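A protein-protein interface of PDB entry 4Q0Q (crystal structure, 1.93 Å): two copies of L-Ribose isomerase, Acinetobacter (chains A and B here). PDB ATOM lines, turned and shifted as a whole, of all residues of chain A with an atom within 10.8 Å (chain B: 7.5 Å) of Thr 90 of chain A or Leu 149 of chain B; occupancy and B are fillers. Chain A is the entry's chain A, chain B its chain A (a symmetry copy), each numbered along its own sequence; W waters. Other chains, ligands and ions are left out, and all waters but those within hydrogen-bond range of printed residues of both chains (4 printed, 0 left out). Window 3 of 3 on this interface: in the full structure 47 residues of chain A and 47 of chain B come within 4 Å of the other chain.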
ATOM      1  N   ALA A  84      12.612  -1.196 -28.972  1.00  0.00           N
ATOM      2  CA  ALA A  84      11.385  -0.510 -29.372  1.00  0.00           C
ATOM      3  C   ALA A  84      10.168  -1.420 -29.156  1.00  0.00           C
ATOM      4  O   ALA A  84       9.218  -1.424 -29.945  1.00  0.00           O
ATOM      5  CB  ALA A  84      11.470  -0.079 -30.829  1.00  0.00           C
ATOM      6  N   VAL A  85      10.206  -2.193 -28.077  1.00  0.00           N
ATOM      7  CA  VAL A  85       9.109  -3.097 -27.757  1.00  0.00           C
ATOM      8  C   VAL A  85       8.020  -2.398 -26.946  1.00  0.00           C
ATOM      9  O   VAL A  85       6.849  -2.775 -27.018  1.00  0.00           O
ATOM     10  CB  VAL A  85       9.628  -4.329 -26.991  1.00  0.00           C
ATOM     11  CG1 VAL A  85       8.473  -5.081 -26.341  1.00  0.00           C
ATOM     12  CG2 VAL A  85      10.370  -5.244 -27.958  1.00  0.00           C
ATOM     13  N   ASP A  86       8.408  -1.378 -26.182  1.00  0.00           N
ATOM     14  CA  ASP A  86       7.455  -0.634 -25.366  1.00  0.00           C
ATOM     15  C   ASP A  86       6.387   0.016 -26.227  1.00  0.00           C
ATOM     16  O   ASP A  86       6.699   0.668 -27.224  1.00  0.00           O
ATOM     17  CB  ASP A  86       8.165   0.452 -24.545  1.00  0.00           C
ATOM     18  CG  ASP A  86       8.956  -0.115 -23.379  1.00  0.00           C
ATOM     19  OD1 ASP A  86      10.091  -0.603 -23.586  1.00  0.00           O
ATOM     20  OD2 ASP A  86       8.432  -0.081 -22.247  1.00  0.00           O
ATOM     21  N   GLY A  87       5.126  -0.167 -25.845  1.00  0.00           N
ATOM     22  CA  GLY A  87       4.034   0.431 -26.592  1.00  0.00           C
ATOM     23  C   GLY A  87       3.500  -0.405 -27.739  1.00  0.00           C
ATOM     24  O   GLY A  87       2.573   0.013 -28.435  1.00  0.00           O
ATOM     25  N   LEU A  88       4.087  -1.577 -27.952  1.00  0.00           N
ATOM     26  CA  LEU A  88       3.644  -2.467 -29.021  1.00  0.00           C
ATOM     27  C   LEU A  88       2.472  -3.327 -28.577  1.00  0.00           C
ATOM     28  O   LEU A  88       2.434  -3.791 -27.438  1.00  0.00           O
ATOM     29  CB  LEU A  88       4.764  -3.426 -29.442  1.00  0.00           C
ATOM     30  CG  LEU A  88       5.942  -2.993 -30.308  1.00  0.00           C
ATOM     31  CD1 LEU A  88       6.841  -4.211 -30.545  1.00  0.00           C
ATOM     32  CD2 LEU A  88       5.448  -2.433 -31.628  1.00  0.00           C
ATOM     33  N   PRO A  89       1.488  -3.537 -29.464  1.00  0.00           N
ATOM     34  CA  PRO A  89       0.362  -4.382 -29.060  1.00  0.00           C
ATOM     35  C   PRO A  89       0.953  -5.779 -28.901  1.00  0.00           C
ATOM     36  O   PRO A  89       1.807  -6.179 -29.693  1.00  0.00           O
ATOM     37  CB  PRO A  89      -0.596  -4.273 -30.242  1.00  0.00           C
ATOM     38  CG  PRO A  89       0.312  -4.005 -31.399  1.00  0.00           C
ATOM     39  CD  PRO A  89       1.284  -3.003 -30.818  1.00  0.00           C
ATOM     40  N   THR A  90       0.521  -6.505 -27.875  1.00  0.00           N
ATOM     41  CA  THR A  90       1.042  -7.842 -27.601  1.00  0.00           C
ATOM     42  C   THR A  90       1.077  -8.770 -28.816  1.00  0.00           C
ATOM     43  O   THR A  90       1.907  -9.674 -28.889  1.00  0.00           O
ATOM     44  CB  THR A  90       0.231  -8.534 -26.471  1.00  0.00           C
ATOM     45  OG1 THR A  90      -1.107  -8.777 -26.919  1.00  0.00           O
ATOM     46  CG2 THR A  90       0.187  -7.650 -25.226  1.00  0.00           C
ATOM     47  N   GLY A  91       0.179  -8.544 -29.768  1.00  0.00           N
ATOM     48  CA  GLY A  91       0.139  -9.382 -30.950  1.00  0.00           C
ATOM     49  C   GLY A  91       1.382  -9.286 -31.818  1.00  0.00           C
ATOM     50  O   GLY A  91       1.645 -10.173 -32.631  1.00  0.00           O
ATOM     51  N   ALA A  92       2.151  -8.214 -31.644  1.00  0.00           N
ATOM     52  CA  ALA A  92       3.360  -8.010 -32.432  1.00  0.00           C
ATOM     53  C   ALA A  92       4.591  -8.637 -31.787  1.00  0.00           C
ATOM     54  O   ALA A  92       5.679  -8.600 -32.353  1.00  0.00           O
ATOM     55  CB  ALA A  92       3.591  -6.516 -32.652  1.00  0.00           C
ATOM     56  N   ALA A  93       4.415  -9.217 -30.607  1.00  0.00           N
ATOM     57  CA  ALA A  93       5.521  -9.835 -29.886  1.00  0.00           C
ATOM     58  C   ALA A  93       6.417 -10.708 -30.761  1.00  0.00           C
ATOM     59  O   ALA A  93       7.637 -10.542 -30.775  1.00  0.00           O
ATOM     60  CB  ALA A  93       4.988 -10.649 -28.717  1.00  0.00           C
ATOM     61  N   PRO A  94       5.830 -11.654 -31.504  1.00  0.00           N
ATOM     62  CA  PRO A  94       6.671 -12.506 -32.348  1.00  0.00           C
ATOM     63  C   PRO A  94       7.339 -11.778 -33.523  1.00  0.00           C
ATOM     64  O   PRO A  94       8.256 -12.310 -34.142  1.00  0.00           O
ATOM     65  CB  PRO A  94       5.699 -13.591 -32.807  1.00  0.00           C
ATOM     66  CG  PRO A  94       4.405 -12.843 -32.907  1.00  0.00           C
ATOM     67  CD  PRO A  94       4.404 -12.001 -31.651  1.00  0.00           C
ATOM     68  N   TYR A  95       6.896 -10.559 -33.817  1.00  0.00           N
ATOM     69  CA  TYR A  95       7.461  -9.809 -34.934  1.00  0.00           C
ATOM     70  C   TYR A  95       8.338  -8.627 -34.523  1.00  0.00           C
ATOM     71  O   TYR A  95       8.923  -7.952 -35.374  1.00  0.00           O
ATOM     72  CB  TYR A  95       6.333  -9.320 -35.842  1.00  0.00           C
ATOM     73  CG  TYR A  95       5.416 -10.432 -36.290  1.00  0.00           C
ATOM     74  CD1 TYR A  95       5.917 -11.538 -36.980  1.00  0.00           C
ATOM     75  CD2 TYR A  95       4.050 -10.395 -36.006  1.00  0.00           C
ATOM     76  CE1 TYR A  95       5.084 -12.580 -37.376  1.00  0.00           C
ATOM     77  CE2 TYR A  95       3.204 -11.432 -36.398  1.00  0.00           C
ATOM     78  CZ  TYR A  95       3.728 -12.520 -37.081  1.00  0.00           C
ATOM     79  OH  TYR A  95       2.900 -13.548 -37.468  1.00  0.00           O
ATOM     80  N   ALA A  96       8.447  -8.389 -33.222  1.00  0.00           N
ATOM     81  CA  ALA A  96       9.246  -7.277 -32.719  1.00  0.00           C
ATOM     82  C   ALA A  96      10.722  -7.387 -33.113  1.00  0.00           C
ATOM     83  O   ALA A  96      11.389  -6.378 -33.338  1.00  0.00           O
ATOM     84  CB  ALA A  96       9.111  -7.185 -31.195  1.00  0.00           C
ATOM     85  N   GLU A  97      11.222  -8.614 -33.205  1.00  0.00           N
ATOM     86  CA  GLU A  97      12.614  -8.850 -33.543  1.00  0.00           C
ATOM     87  C   GLU A  97      13.030  -8.328 -34.920  1.00  0.00           C
ATOM     88  O   GLU A  97      14.219  -8.285 -35.233  1.00  0.00           O
ATOM     89  CB  GLU A  97      12.922 -10.345 -33.428  1.00  0.00           C
ATOM     90  CG  GLU A  97      12.083 -11.229 -34.329  1.00  0.00           C
ATOM     91  CD  GLU A  97      12.077 -12.670 -33.865  1.00  0.00           C
ATOM     92  OE1 GLU A  97      11.532 -12.936 -32.776  1.00  0.00           O
ATOM     93  OE2 GLU A  97      12.624 -13.535 -34.576  1.00  0.00           O
ATOM     94  N   PRO A 233      14.171  -8.248 -23.866  1.00  0.00           N
ATOM     95  CA  PRO A 233      12.819  -7.681 -23.816  1.00  0.00           C
ATOM     96  C   PRO A 233      11.737  -8.730 -24.047  1.00  0.00           C
ATOM     97  O   PRO A 233      10.616  -8.607 -23.551  1.00  0.00           O
ATOM     98  CB  PRO A 233      12.852  -6.626 -24.917  1.00  0.00           C
ATOM     99  CG  PRO A 233      13.799  -7.220 -25.909  1.00  0.00           C
ATOM    100  CD  PRO A 233      14.912  -7.722 -25.026  1.00  0.00           C
ATOM    101  N   ILE A 234      12.086  -9.755 -24.814  1.00  0.00           N
ATOM    102  CA  ILE A 234      11.174 -10.845 -25.123  1.00  0.00           C
ATOM    103  C   ILE A 234      11.982 -12.138 -25.064  1.00  0.00           C
ATOM    104  O   ILE A 234      13.085 -12.213 -25.604  1.00  0.00           O
ATOM    105  CB  ILE A 234      10.543 -10.659 -26.521  1.00  0.00           C
ATOM    106  CG1 ILE A 234       9.593  -9.459 -26.493  1.00  0.00           C
ATOM    107  CG2 ILE A 234       9.803 -11.920 -26.942  1.00  0.00           C
ATOM    108  CD1 ILE A 234       8.921  -9.163 -27.815  1.00  0.00           C
ATOM    109  N   PRO A 235      11.440 -13.168 -24.393  1.00  0.00           N
ATOM    110  CA  PRO A 235      12.068 -14.482 -24.221  1.00  0.00           C
ATOM    111  C   PRO A 235      12.970 -14.959 -25.355  1.00  0.00           C
ATOM    112  O   PRO A 235      14.171 -15.163 -25.159  1.00  0.00           O
ATOM    113  CB  PRO A 235      10.872 -15.398 -24.005  1.00  0.00           C
ATOM    114  CG  PRO A 235       9.972 -14.534 -23.186  1.00  0.00           C
ATOM    115  CD  PRO A 235      10.046 -13.199 -23.910  1.00  0.00           C
ATOM    116  N   TRP A 237      14.351 -13.520 -27.863  1.00  0.00           N
ATOM    117  CA  TRP A 237      15.505 -12.676 -28.153  1.00  0.00           C
ATOM    118  C   TRP A 237      16.796 -13.113 -27.469  1.00  0.00           C
ATOM    119  O   TRP A 237      17.874 -13.032 -28.057  1.00  0.00           O
ATOM    120  CB  TRP A 237      15.196 -11.235 -27.757  1.00  0.00           C
ATOM    121  CG  TRP A 237      14.157 -10.583 -28.613  1.00  0.00           C
ATOM    122  CD1 TRP A 237      13.014 -11.152 -29.103  1.00  0.00           C
ATOM    123  CD2 TRP A 237      14.141  -9.218 -29.037  1.00  0.00           C
ATOM    124  NE1 TRP A 237      12.288 -10.220 -29.805  1.00  0.00           N
ATOM    125  CE2 TRP A 237      12.957  -9.025 -29.779  1.00  0.00           C
ATOM    126  CE3 TRP A 237      15.013  -8.136 -28.858  1.00  0.00           C
ATOM    127  CZ2 TRP A 237      12.618  -7.792 -30.342  1.00  0.00           C
ATOM    128  CZ3 TRP A 237      14.676  -6.911 -29.416  1.00  0.00           C
ATOM    129  CH2 TRP A 237      13.488  -6.750 -30.150  1.00  0.00           C
ATOM    130  N   TYR B  95       1.657  -5.471 -38.261  1.00  0.00           N
ATOM    131  CA  TYR B  95       2.543  -4.848 -37.283  1.00  0.00           C
ATOM    132  C   TYR B  95       3.721  -4.087 -37.891  1.00  0.00           C
ATOM    133  O   TYR B  95       4.507  -3.466 -37.172  1.00  0.00           O
ATOM    134  CB  TYR B  95       3.064  -5.912 -36.317  1.00  0.00           C
ATOM    135  CG  TYR B  95       1.957  -6.714 -35.676  1.00  0.00           C
ATOM    136  CD1 TYR B  95       0.953  -6.084 -34.937  1.00  0.00           C
ATOM    137  CD2 TYR B  95       1.897  -8.100 -35.823  1.00  0.00           C
ATOM    138  CE1 TYR B  95      -0.084  -6.812 -34.361  1.00  0.00           C
ATOM    139  CE2 TYR B  95       0.863  -8.841 -35.251  1.00  0.00           C
ATOM    140  CZ  TYR B  95      -0.122  -8.191 -34.523  1.00  0.00           C
ATOM    141  OH  TYR B  95      -1.147  -8.915 -33.959  1.00  0.00           O
ATOM    142  N   TYR B  98       4.716  -0.323 -37.132  1.00  0.00           N
ATOM    143  CA  TYR B  98       5.386   0.032 -35.882  1.00  0.00           C
ATOM    144  C   TYR B  98       6.900  -0.006 -36.072  1.00  0.00           C
ATOM    145  O   TYR B  98       7.655   0.429 -35.202  1.00  0.00           O
ATOM    146  CB  TYR B  98       5.005  -0.953 -34.777  1.00  0.00           C
ATOM    147  CG  TYR B  98       3.572  -0.839 -34.322  1.00  0.00           C
ATOM    148  CD1 TYR B  98       3.207   0.075 -33.333  1.00  0.00           C
ATOM    149  CD2 TYR B  98       2.574  -1.623 -34.902  1.00  0.00           C
ATOM    150  CE1 TYR B  98       1.877   0.206 -32.931  1.00  0.00           C
ATOM    151  CE2 TYR B  98       1.244  -1.497 -34.512  1.00  0.00           C
ATOM    152  CZ  TYR B  98       0.902  -0.582 -33.527  1.00  0.00           C
ATOM    153  OH  TYR B  98      -0.414  -0.446 -33.152  1.00  0.00           O
ATOM    154  N   GLY B 120       1.291   6.866 -32.018  1.00  0.00           N
ATOM    155  CA  GLY B 120       0.781   5.582 -31.590  1.00  0.00           C
ATOM    156  C   GLY B 120       1.705   4.462 -32.029  1.00  0.00           C
ATOM    157  O   GLY B 120       1.810   3.437 -31.357  1.00  0.00           O
ATOM    158  N   PRO B 141       2.968   6.610 -20.412  1.00  0.00           N
ATOM    159  CA  PRO B 141       2.493   6.436 -21.787  1.00  0.00           C
ATOM    160  C   PRO B 141       0.968   6.499 -21.816  1.00  0.00           C
ATOM    161  O   PRO B 141       0.315   6.355 -20.781  1.00  0.00           O
ATOM    162  CB  PRO B 141       3.015   5.052 -22.154  1.00  0.00           C
ATOM    163  CG  PRO B 141       2.936   4.318 -20.852  1.00  0.00           C
ATOM    164  CD  PRO B 141       3.487   5.341 -19.867  1.00  0.00           C
ATOM    165  N   SER B 142       0.401   6.734 -22.992  1.00  0.00           N
ATOM    166  CA  SER B 142      -1.046   6.762 -23.115  1.00  0.00           C
ATOM    167  C   SER B 142      -1.476   5.308 -23.306  1.00  0.00           C
ATOM    168  O   SER B 142      -0.650   4.441 -23.600  1.00  0.00           O
ATOM    169  CB  SER B 142      -1.465   7.590 -24.326  1.00  0.00           C
ATOM    170  OG  SER B 142      -1.014   6.981 -25.520  1.00  0.00           O
ATOM    171  N   ALA B 143      -2.761   5.037 -23.131  1.00  0.00           N
ATOM    172  CA  ALA B 143      -3.263   3.682 -23.297  1.00  0.00           C
ATOM    173  C   ALA B 143      -4.041   3.615 -24.595  1.00  0.00           C
ATOM    174  O   ALA B 143      -4.328   4.641 -25.207  1.00  0.00           O
ATOM    175  CB  ALA B 143      -4.168   3.311 -22.128  1.00  0.00           C
ATOM    176  N   GLU B 144      -4.375   2.405 -25.024  1.00  0.00           N
ATOM    177  CA  GLU B 144      -5.148   2.239 -26.243  1.00  0.00           C
ATOM    178  C   GLU B 144      -6.311   1.295 -25.965  1.00  0.00           C
ATOM    179  O   GLU B 144      -6.145   0.078 -25.880  1.00  0.00           O
ATOM    180  CB  GLU B 144      -4.270   1.702 -27.370  1.00  0.00           C
ATOM    181  CG  GLU B 144      -4.941   1.765 -28.729  1.00  0.00           C
ATOM    182  CD  GLU B 144      -3.972   1.536 -29.863  1.00  0.00           C
ATOM    183  OE1 GLU B 144      -3.337   0.462 -29.893  1.00  0.00           O
ATOM    184  OE2 GLU B 144      -3.843   2.433 -30.720  1.00  0.00           O
ATOM    185  N   SER B 145      -7.490   1.887 -25.813  1.00  0.00           N
ATOM    186  CA  SER B 145      -8.720   1.163 -25.523  1.00  0.00           C
ATOM    187  C   SER B 145      -8.863  -0.179 -26.239  1.00  0.00           C
ATOM    188  O   SER B 145      -8.807  -0.249 -27.468  1.00  0.00           O
ATOM    189  CB  SER B 145      -9.920   2.048 -25.866  1.00  0.00           C
ATOM    190  OG  SER B 145     -11.129   1.471 -25.406  1.00  0.00           O
ATOM    191  N   VAL B 147      -6.817  -2.801 -26.307  1.00  0.00           N
ATOM    192  CA  VAL B 147      -5.615  -3.543 -26.671  1.00  0.00           C
ATOM    193  C   VAL B 147      -4.515  -3.536 -25.619  1.00  0.00           C
ATOM    194  O   VAL B 147      -4.158  -2.489 -25.073  1.00  0.00           O
ATOM    195  CB  VAL B 147      -5.041  -3.032 -28.012  1.00  0.00           C
ATOM    196  CG1 VAL B 147      -4.912  -1.527 -27.979  1.00  0.00           C
ATOM    197  CG2 VAL B 147      -3.690  -3.683 -28.286  1.00  0.00           C
ATOM    198  N   GLU B 148      -3.986  -4.726 -25.344  1.00  0.00           N
ATOM    199  CA  GLU B 148      -2.913  -4.911 -24.374  1.00  0.00           C
ATOM    200  C   GLU B 148      -1.619  -4.467 -25.053  1.00  0.00           C
ATOM    201  O   GLU B 148      -1.449  -4.655 -26.259  1.00  0.00           O
ATOM    202  CB  GLU B 148      -2.816  -6.386 -23.978  1.00  0.00           C
ATOM    203  CG  GLU B 148      -2.702  -6.650 -22.477  1.00  0.00           C
ATOM    204  CD  GLU B 148      -1.376  -6.205 -21.883  1.00  0.00           C
ATOM    205  OE1 GLU B 148      -1.079  -4.991 -21.921  1.00  0.00           O
ATOM    206  OE2 GLU B 148      -0.629  -7.071 -21.373  1.00  0.00           O
ATOM    207  N   LEU B 149      -0.713  -3.880 -24.279  1.00  0.00           N
ATOM    208  CA  LEU B 149       0.552  -3.398 -24.818  1.00  0.00           C
ATOM    209  C   LEU B 149       1.736  -3.988 -24.073  1.00  0.00           C
ATOM    210  O   LEU B 149       1.641  -4.306 -22.888  1.00  0.00           O
ATOM    211  CB  LEU B 149       0.599  -1.868 -24.739  1.00  0.00           C
ATOM    212  CG  LEU B 149      -0.557  -1.161 -25.455  1.00  0.00           C
ATOM    213  CD1 LEU B 149      -0.528   0.325 -25.153  1.00  0.00           C
ATOM    214  CD2 LEU B 149      -0.460  -1.405 -26.945  1.00  0.00           C
ATOM    215  N   LEU B 150       2.854  -4.135 -24.774  1.00  0.00           N
ATOM    216  CA  LEU B 150       4.060  -4.673 -24.167  1.00  0.00           C
ATOM    217  C   LEU B 150       4.817  -3.591 -23.402  1.00  0.00           C
ATOM    218  O   LEU B 150       4.614  -2.394 -23.627  1.00  0.00           O
ATOM    219  CB  LEU B 150       4.974  -5.274 -25.239  1.00  0.00           C
ATOM    220  CG  LEU B 150       4.421  -6.457 -26.037  1.00  0.00           C
ATOM    221  CD1 LEU B 150       5.455  -6.913 -27.050  1.00  0.00           C
ATOM    222  CD2 LEU B 150       4.069  -7.598 -25.094  1.00  0.00           C
ATOM    223  N   ASN B 151       5.682  -4.026 -22.491  1.00  0.00           N
ATOM    224  CA  ASN B 151       6.492  -3.119 -21.689  1.00  0.00           C
ATOM    225  C   ASN B 151       7.869  -3.733 -21.491  1.00  0.00           C
ATOM    226  O   ASN B 151       8.002  -4.954 -21.398  1.00  0.00           O
ATOM    227  CB  ASN B 151       5.848  -2.886 -20.319  1.00  0.00           C
ATOM    228  CG  ASN B 151       4.518  -2.171 -20.417  1.00  0.00           C
ATOM    229  OD1 ASN B 151       4.442  -1.041 -20.903  1.00  0.00           O
ATOM    230  ND2 ASN B 151       3.458  -2.826 -19.954  1.00  0.00           N
ATOM    231  N   ARG B 195       7.059   5.294 -28.249  1.00  0.00           N
ATOM    232  CA  ARG B 195       5.776   5.590 -28.861  1.00  0.00           C
ATOM    233  C   ARG B 195       4.746   5.695 -27.735  1.00  0.00           C
ATOM    234  O   ARG B 195       4.928   5.124 -26.659  1.00  0.00           O
ATOM    235  CB  ARG B 195       5.388   4.463 -29.824  1.00  0.00           C
ATOM    236  CG  ARG B 195       5.337   3.085 -29.164  1.00  0.00           C
ATOM    237  CD  ARG B 195       4.880   2.016 -30.138  1.00  0.00           C
ATOM    238  NE  ARG B 195       5.851   1.756 -31.196  1.00  0.00           N
ATOM    239  CZ  ARG B 195       6.832   0.865 -31.109  1.00  0.00           C
ATOM    240  NH1 ARG B 195       6.976   0.143 -30.008  1.00  0.00           N
ATOM    241  NH2 ARG B 195       7.659   0.686 -32.132  1.00  0.00           N
ATOM    242  N   LYS B 196       3.675   6.435 -27.995  1.00  0.00           N
ATOM    243  CA  LYS B 196       2.591   6.644 -27.039  1.00  0.00           C
ATOM    244  C   LYS B 196       2.938   7.562 -25.876  1.00  0.00           C
ATOM    245  O   LYS B 196       2.209   7.621 -24.890  1.00  0.00           O
ATOM    246  CB  LYS B 196       2.057   5.303 -26.519  1.00  0.00           C
ATOM    247  CG  LYS B 196       1.363   4.475 -27.597  1.00  0.00           C
ATOM    248  CD  LYS B 196       0.778   3.188 -27.037  1.00  0.00           C
ATOM    249  CE  LYS B 196       0.016   2.419 -28.103  1.00  0.00           C
ATOM    250  NZ  LYS B 196       0.909   1.928 -29.184  1.00  0.00           N
HETATM  251  O   HOH W   1       9.216   1.737 -28.140  1.00  0.00           O
HETATM  252  O   HOH W   2       6.430   1.115 -21.212  1.00  0.00           O
HETATM  253  O   HOH W   3       4.994   3.031 -24.617  1.00  0.00           O
HETATM  254  O   HOH W   4       8.696  -2.267 -33.023  1.00  0.00           O
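Water W2 bridges OD2 of Asp 86 of chain A (2.6 Å) and OD1 of Asn 151 of chain B (2.9 Å). Water W1 lies within hydrogen-bond range of the backbone carbonyl oxygen of Asp 86 of chain A (2.9 Å) and the guanidinium group of Arg 195 of chain B (3.3 Å). Water W3 lies within hydrogen-bond range of the backbone carbonyl oxygen of Arg 195 of chain B and the backbone NH of Gly 87 of chain A. Water W4 bridges O of Ala 84 of chain A and NH2 of Arg 195 of chain B.
Tyr 95 of chain B touches its own counterpart, Tyr 95 of chain A. 1 position is printed for both chains. Of the 23 pairs that touch across the chains among the printed residues, 1 has its exchanged pair printed and touching as well.
Hydrophobic or aromatic side chains of chain A that line the printed part of chain B: Val 85, Leu 88, Pro 89, Ala 92 and Tyr 95. Among the printed residues, 23 pairs touch across the chains. Among the printed residues, no Asp or Glu carboxylate lies within 4 Å of a Lys or Arg side-chain nitrogen of the other chain.
The backbone carbonyl oxygen (O) of Gly 120 of chain B lies within hydrogen-bond range of the side-chain amino group (NZ) of Lys 196 of chain B (2.8 Å). O of Tyr 98 of chain B lies within hydrogen-bond range of NH2 of Arg 195 of chain B (3.1 Å). The backbone NH (N) of Ser 142 of chain B lies within hydrogen-bond range of the backbone carbonyl oxygen (O) of Lys 196 of chain B.
Printed residues of chain A within 4 Å of Leu 149 of chain B: Gly 87 (3.7 Å), Leu 88 (3.2 Å), Pro 89 (3.7 Å) and Thr 90 (3.99 Å). No residue of chain A comes within 4 Å of Ala 143 of chain B. No residue of chain A comes within 4 Å of Glu 144 of chain B. Of chain A, only Pro 89 (3.7 Å) comes within 4 Å of Val 147 of chain B. Asn 151 of chain B touches just one residue of chain A: Asp 86 (3.6 Å). Of the printed residues of chain B, Gly 87 of chain A touches Leu 149, Leu 150, Arg 195 and Lys 196. Printed residues of chain B within 4 Å of Leu 88 of chain A: Tyr 98, Leu 149, Leu 150 and Arg 195. Printed residues of chain B within 4 Å of Pro 89 of chain A: Tyr 98 (3.7 Å), Val 147 (3.7 Å), Glu 148 (3.3 Å) and Leu 149 (3.7 Å). Printed residues of chain A within 4 Å of Arg 195 of chain B: Ala 84, Asp 86, Gly 87 and Leu 88. Ser 145 of chain B touches none of the printed residues of chain A. The nearest printed residue of chain B that does not touch Thr 90 of chain A is Val 147 of chain B (5.1 Å).
Leu 150 of chain B touches Val 85 of chain A. Asp 86 of chain A touches Leu 150 of chain B (CA to O, 3.8 Å). Asp 86 of chain A touches Asn 151 of chain B (OD2 to CA, 3.6 Å). Tyr 98 of chain B touches Leu 88 of chain A. O of Leu 88 of chain A touches CA of Leu 149 of chain B, at 3.2 Å. CG of Leu 88 of chain A touches NH1 of Arg 195 of chain B (3.3 Å). Pro 89 of chain A touches Tyr 98 of chain B. Pro 89 of chain A touches Val 147 of chain B. Thr 90 of chain A touches Leu 149 of chain B (CG2 to N, 3.99 Å). CD2 of Tyr 95 of chain A touches CD2 of Tyr 95 of chain B (3.2 Å).
NZ of Lys 196 of chain B lies within hydrogen-bond range of O of Gly 87 of chain A (2.6 Å). The backbone carbonyl oxygen (O) of Ala 84 of chain A sits at hydrogen-bond distance from the guanidinium group (NH1) of Arg 195 of chain B, 2.7 Å away. NH1 of Arg 195 of chain B lies within hydrogen-bond range of O of Asp 86 of chain A, 2.8 Å away. The backbone carbonyl oxygen (O) of Leu 88 of chain A lies within hydrogen-bond range of the backbone NH (N) of Leu 150 of chain B. The backbone carbonyl oxygen (O) of Glu 148 of chain B lies within hydrogen-bond range of the backbone NH (N) of Thr 90 of chain A (3.1 Å). The backbone carbonyl oxygen of Gly 91 of chain A lies close to the side-chain hydroxyl of Tyr 95 of chain B, at 3.3 Å. N of Gly 87 of chain A sits at hydrogen-bond distance from O of Leu 150 of chain B (3.2 Å).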
